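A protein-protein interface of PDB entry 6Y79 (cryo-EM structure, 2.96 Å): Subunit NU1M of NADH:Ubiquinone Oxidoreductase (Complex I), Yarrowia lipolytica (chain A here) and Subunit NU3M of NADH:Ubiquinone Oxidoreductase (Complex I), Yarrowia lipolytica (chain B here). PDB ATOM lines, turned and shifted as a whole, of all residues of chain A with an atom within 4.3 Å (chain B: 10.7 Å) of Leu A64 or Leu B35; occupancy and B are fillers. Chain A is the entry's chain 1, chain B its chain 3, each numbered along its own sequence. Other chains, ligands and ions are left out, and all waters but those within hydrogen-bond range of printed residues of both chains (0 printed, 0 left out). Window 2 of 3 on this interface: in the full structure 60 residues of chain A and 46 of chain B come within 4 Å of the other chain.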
ATOM      1  N   ILE A  62     -23.856  24.571 -24.046  1.00  0.00           N
ATOM      2  CA  ILE A  62     -22.824  23.623 -24.462  1.00  0.00           C
ATOM      3  C   ILE A  62     -23.401  22.725 -25.548  1.00  0.00           C
ATOM      4  O   ILE A  62     -24.461  22.116 -25.373  1.00  0.00           O
ATOM      5  CB  ILE A  62     -22.310  22.784 -23.281  1.00  0.00           C
ATOM      6  CG1 ILE A  62     -21.736  23.670 -22.178  1.00  0.00           C
ATOM      7  CG2 ILE A  62     -21.250  21.805 -23.731  1.00  0.00           C
ATOM      8  CD1 ILE A  62     -22.653  23.818 -20.985  1.00  0.00           C
ATOM      9  N   VAL A  63     -22.705  22.633 -26.669  1.00  0.00           N
ATOM     10  CA  VAL A  63     -23.160  21.856 -27.810  1.00  0.00           C
ATOM     11  C   VAL A  63     -22.243  20.639 -27.954  1.00  0.00           C
ATOM     12  O   VAL A  63     -21.023  20.768 -28.053  1.00  0.00           O
ATOM     13  CB  VAL A  63     -23.269  22.738 -29.073  1.00  0.00           C
ATOM     14  CG1 VAL A  63     -24.314  23.850 -28.807  1.00  0.00           C
ATOM     15  CG2 VAL A  63     -21.972  23.424 -29.480  1.00  0.00           C
ATOM     16  N   LEU A  64     -22.816  19.447 -27.851  1.00  0.00           N
ATOM     17  CA  LEU A  64     -22.071  18.208 -28.054  1.00  0.00           C
ATOM     18  C   LEU A  64     -22.494  17.624 -29.393  1.00  0.00           C
ATOM     19  O   LEU A  64     -23.638  17.179 -29.517  1.00  0.00           O
ATOM     20  CB  LEU A  64     -22.291  17.207 -26.906  1.00  0.00           C
ATOM     21  CG  LEU A  64     -23.525  16.495 -26.326  1.00  0.00           C
ATOM     22  CD1 LEU A  64     -23.782  15.110 -26.953  1.00  0.00           C
ATOM     23  CD2 LEU A  64     -23.398  16.416 -24.786  1.00  0.00           C
ATOM     24  N   PRO A  65     -21.654  17.666 -30.438  1.00  0.00           N
ATOM     25  CA  PRO A  65     -22.140  17.361 -31.793  1.00  0.00           C
ATOM     26  C   PRO A  65     -22.437  15.884 -32.017  1.00  0.00           C
ATOM     27  O   PRO A  65     -22.085  15.005 -31.226  1.00  0.00           O
ATOM     28  CB  PRO A  65     -21.018  17.855 -32.720  1.00  0.00           C
ATOM     29  CG  PRO A  65     -19.852  18.063 -31.860  1.00  0.00           C
ATOM     30  CD  PRO A  65     -20.369  18.389 -30.497  1.00  0.00           C
ATOM     31  N   LYS A  66     -23.114  15.638 -33.154  1.00  0.00           N
ATOM     32  CA  LYS A  66     -23.430  14.296 -33.646  1.00  0.00           C
ATOM     33  C   LYS A  66     -22.180  13.432 -33.769  1.00  0.00           C
ATOM     34  O   LYS A  66     -22.249  12.214 -33.615  1.00  0.00           O
ATOM     35  CB  LYS A  66     -24.064  14.374 -35.024  1.00  0.00           C
ATOM     36  CG  LYS A  66     -25.257  15.277 -35.220  1.00  0.00           C
ATOM     37  CD  LYS A  66     -25.544  15.324 -36.715  1.00  0.00           C
ATOM     38  CE  LYS A  66     -26.711  16.210 -37.034  1.00  0.00           C
ATOM     39  NZ  LYS A  66     -27.936  15.576 -36.500  1.00  0.00           N
ATOM     40  N   ILE B  23     -22.711  23.484 -16.485  1.00  0.00           N
ATOM     41  CA  ILE B  23     -23.648  22.409 -16.787  1.00  0.00           C
ATOM     42  C   ILE B  23     -24.885  22.520 -15.904  1.00  0.00           C
ATOM     43  O   ILE B  23     -26.004  22.373 -16.377  1.00  0.00           O
ATOM     44  CB  ILE B  23     -22.941  21.047 -16.642  1.00  0.00           C
ATOM     45  CG1 ILE B  23     -21.927  20.833 -17.772  1.00  0.00           C
ATOM     46  CG2 ILE B  23     -23.923  19.901 -16.672  1.00  0.00           C
ATOM     47  CD1 ILE B  23     -21.076  19.586 -17.599  1.00  0.00           C
ATOM     48  N   VAL B  27     -28.429  26.794 -20.419  1.00  0.00           N
ATOM     49  CA  VAL B  27     -29.480  26.196 -21.230  1.00  0.00           C
ATOM     50  C   VAL B  27     -28.908  25.058 -22.070  1.00  0.00           C
ATOM     51  O   VAL B  27     -27.789  25.145 -22.584  1.00  0.00           O
ATOM     52  CB  VAL B  27     -30.085  27.315 -22.103  1.00  0.00           C
ATOM     53  CG1 VAL B  27     -31.079  26.793 -23.102  1.00  0.00           C
ATOM     54  CG2 VAL B  27     -30.708  28.396 -21.223  1.00  0.00           C
ATOM     55  N   TYR B  28     -29.661  23.957 -22.182  1.00  0.00           N
ATOM     56  CA  TYR B  28     -29.242  22.884 -23.075  1.00  0.00           C
ATOM     57  C   TYR B  28     -29.900  23.014 -24.446  1.00  0.00           C
ATOM     58  O   TYR B  28     -29.184  23.198 -25.426  1.00  0.00           O
ATOM     59  CB  TYR B  28     -29.548  21.517 -22.451  1.00  0.00           C
ATOM     60  CG  TYR B  28     -29.141  20.308 -23.282  1.00  0.00           C
ATOM     61  CD1 TYR B  28     -27.833  20.150 -23.740  1.00  0.00           C
ATOM     62  CD2 TYR B  28     -30.056  19.295 -23.553  1.00  0.00           C
ATOM     63  CE1 TYR B  28     -27.464  19.028 -24.481  1.00  0.00           C
ATOM     64  CE2 TYR B  28     -29.702  18.179 -24.286  1.00  0.00           C
ATOM     65  CZ  TYR B  28     -28.410  18.045 -24.745  1.00  0.00           C
ATOM     66  OH  TYR B  28     -28.086  16.922 -25.469  1.00  0.00           O
ATOM     67  N   LYS B  29     -31.231  22.880 -24.496  1.00  0.00           N
ATOM     68  CA  LYS B  29     -32.140  23.135 -25.634  1.00  0.00           C
ATOM     69  C   LYS B  29     -31.603  22.991 -27.040  1.00  0.00           C
ATOM     70  O   LYS B  29     -31.625  23.996 -27.834  1.00  0.00           O
ATOM     71  CB  LYS B  29     -32.844  24.468 -25.437  1.00  0.00           C
ATOM     72  CG  LYS B  29     -33.782  24.552 -24.205  1.00  0.00           C
ATOM     73  CD  LYS B  29     -35.051  23.685 -24.323  1.00  0.00           C
ATOM     74  CE  LYS B  29     -35.001  22.424 -23.464  1.00  0.00           C
ATOM     75  NZ  LYS B  29     -36.252  21.631 -23.622  1.00  0.00           N
ATOM     76  N   PRO B  30     -31.112  21.819 -27.476  1.00  0.00           N
ATOM     77  CA  PRO B  30     -30.549  21.662 -28.815  1.00  0.00           C
ATOM     78  C   PRO B  30     -31.556  21.151 -29.849  1.00  0.00           C
ATOM     79  O   PRO B  30     -32.708  20.889 -29.481  1.00  0.00           O
ATOM     80  CB  PRO B  30     -29.426  20.659 -28.558  1.00  0.00           C
ATOM     81  CG  PRO B  30     -30.017  19.733 -27.544  1.00  0.00           C
ATOM     82  CD  PRO B  30     -31.038  20.535 -26.740  1.00  0.00           C
ATOM     83  N   TYR B  31     -31.143  21.003 -31.116  1.00  0.00           N
ATOM     84  CA  TYR B  31     -31.960  20.403 -32.180  1.00  0.00           C
ATOM     85  C   TYR B  31     -31.059  20.092 -33.375  1.00  0.00           C
ATOM     86  O   TYR B  31     -29.852  20.339 -33.333  1.00  0.00           O
ATOM     87  CB  TYR B  31     -33.140  21.300 -32.588  1.00  0.00           C
ATOM     88  CG  TYR B  31     -32.804  22.686 -33.063  1.00  0.00           C
ATOM     89  CD1 TYR B  31     -32.472  23.703 -32.143  1.00  0.00           C
ATOM     90  CD2 TYR B  31     -32.884  23.022 -34.408  1.00  0.00           C
ATOM     91  CE1 TYR B  31     -32.179  24.979 -32.580  1.00  0.00           C
ATOM     92  CE2 TYR B  31     -32.596  24.300 -34.823  1.00  0.00           C
ATOM     93  CZ  TYR B  31     -32.253  25.254 -33.942  1.00  0.00           C
ATOM     94  OH  TYR B  31     -31.978  26.524 -34.400  1.00  0.00           O
ATOM     95  N   ASN B  32     -31.662  19.583 -34.461  1.00  0.00           N
ATOM     96  CA  ASN B  32     -30.915  19.021 -35.591  1.00  0.00           C
ATOM     97  C   ASN B  32     -30.046  20.068 -36.282  1.00  0.00           C
ATOM     98  O   ASN B  32     -28.861  19.825 -36.537  1.00  0.00           O
ATOM     99  CB  ASN B  32     -31.884  18.404 -36.605  1.00  0.00           C
ATOM    100  CG  ASN B  32     -32.610  17.182 -36.071  1.00  0.00           C
ATOM    101  OD1 ASN B  32     -32.008  16.284 -35.478  1.00  0.00           O
ATOM    102  ND2 ASN B  32     -33.921  17.153 -36.271  1.00  0.00           N
ATOM    103  N   GLU B  33     -30.619  21.239 -36.586  1.00  0.00           N
ATOM    104  CA  GLU B  33     -29.900  22.263 -37.325  1.00  0.00           C
ATOM    105  C   GLU B  33     -28.764  22.874 -36.511  1.00  0.00           C
ATOM    106  O   GLU B  33     -27.826  23.427 -37.091  1.00  0.00           O
ATOM    107  CB  GLU B  33     -30.855  23.355 -37.706  1.00  0.00           C
ATOM    108  CG  GLU B  33     -32.091  22.947 -38.427  1.00  0.00           C
ATOM    109  CD  GLU B  33     -31.921  22.884 -39.908  1.00  0.00           C
ATOM    110  OE1 GLU B  33     -31.055  23.611 -40.426  1.00  0.00           O
ATOM    111  OE2 GLU B  33     -32.697  22.156 -40.552  1.00  0.00           O
ATOM    112  N   LYS B  34     -28.870  22.858 -35.180  1.00  0.00           N
ATOM    113  CA  LYS B  34     -27.794  23.372 -34.340  1.00  0.00           C
ATOM    114  C   LYS B  34     -26.661  22.364 -34.256  1.00  0.00           C
ATOM    115  O   LYS B  34     -25.484  22.731 -34.266  1.00  0.00           O
ATOM    116  CB  LYS B  34     -28.331  23.699 -32.949  1.00  0.00           C
ATOM    117  CG  LYS B  34     -27.302  24.253 -31.988  1.00  0.00           C
ATOM    118  CD  LYS B  34     -27.909  24.425 -30.612  1.00  0.00           C
ATOM    119  CE  LYS B  34     -29.132  25.323 -30.663  1.00  0.00           C
ATOM    120  NZ  LYS B  34     -29.674  25.661 -29.320  1.00  0.00           N
ATOM    121  N   LEU B  35     -27.009  21.091 -34.159  1.00  0.00           N
ATOM    122  CA  LEU B  35     -26.045  20.012 -34.142  1.00  0.00           C
ATOM    123  C   LEU B  35     -25.397  19.867 -35.520  1.00  0.00           C
ATOM    124  O   LEU B  35     -25.944  20.294 -36.541  1.00  0.00           O
ATOM    125  CB  LEU B  35     -26.747  18.722 -33.708  1.00  0.00           C
ATOM    126  CG  LEU B  35     -26.898  18.395 -32.216  1.00  0.00           C
ATOM    127  CD1 LEU B  35     -25.544  18.371 -31.786  1.00  0.00           C
ATOM    128  CD2 LEU B  35     -27.583  19.368 -31.326  1.00  0.00           C
ATOM    129  N   GLY B  36     -24.206  19.277 -35.542  1.00  0.00           N
ATOM    130  CA  GLY B  36     -23.453  19.146 -36.777  1.00  0.00           C
ATOM    131  C   GLY B  36     -22.377  20.204 -36.926  1.00  0.00           C
ATOM    132  O   GLY B  36     -22.350  21.178 -36.176  1.00  0.00           O
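Hydrophobic or aromatic side chains of chain B within 4 Å of the printed part of chain A: Leu B35.
No residue of chain B comes within 4 Å of Val A63. Of chain B, only Leu B35 (3.2 Å) comes within 4 Å of Leu A64. Of the printed residues of chain B, Lys A66 touches Leu B35 (3.9 Å). Glu B33 touches none of the printed residues of chain A. Leu B35 touches three residues of chain A.
Leu A64 touches Leu B35. Pro A65 touches Leu B35. Lys A66 touches Leu B35.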
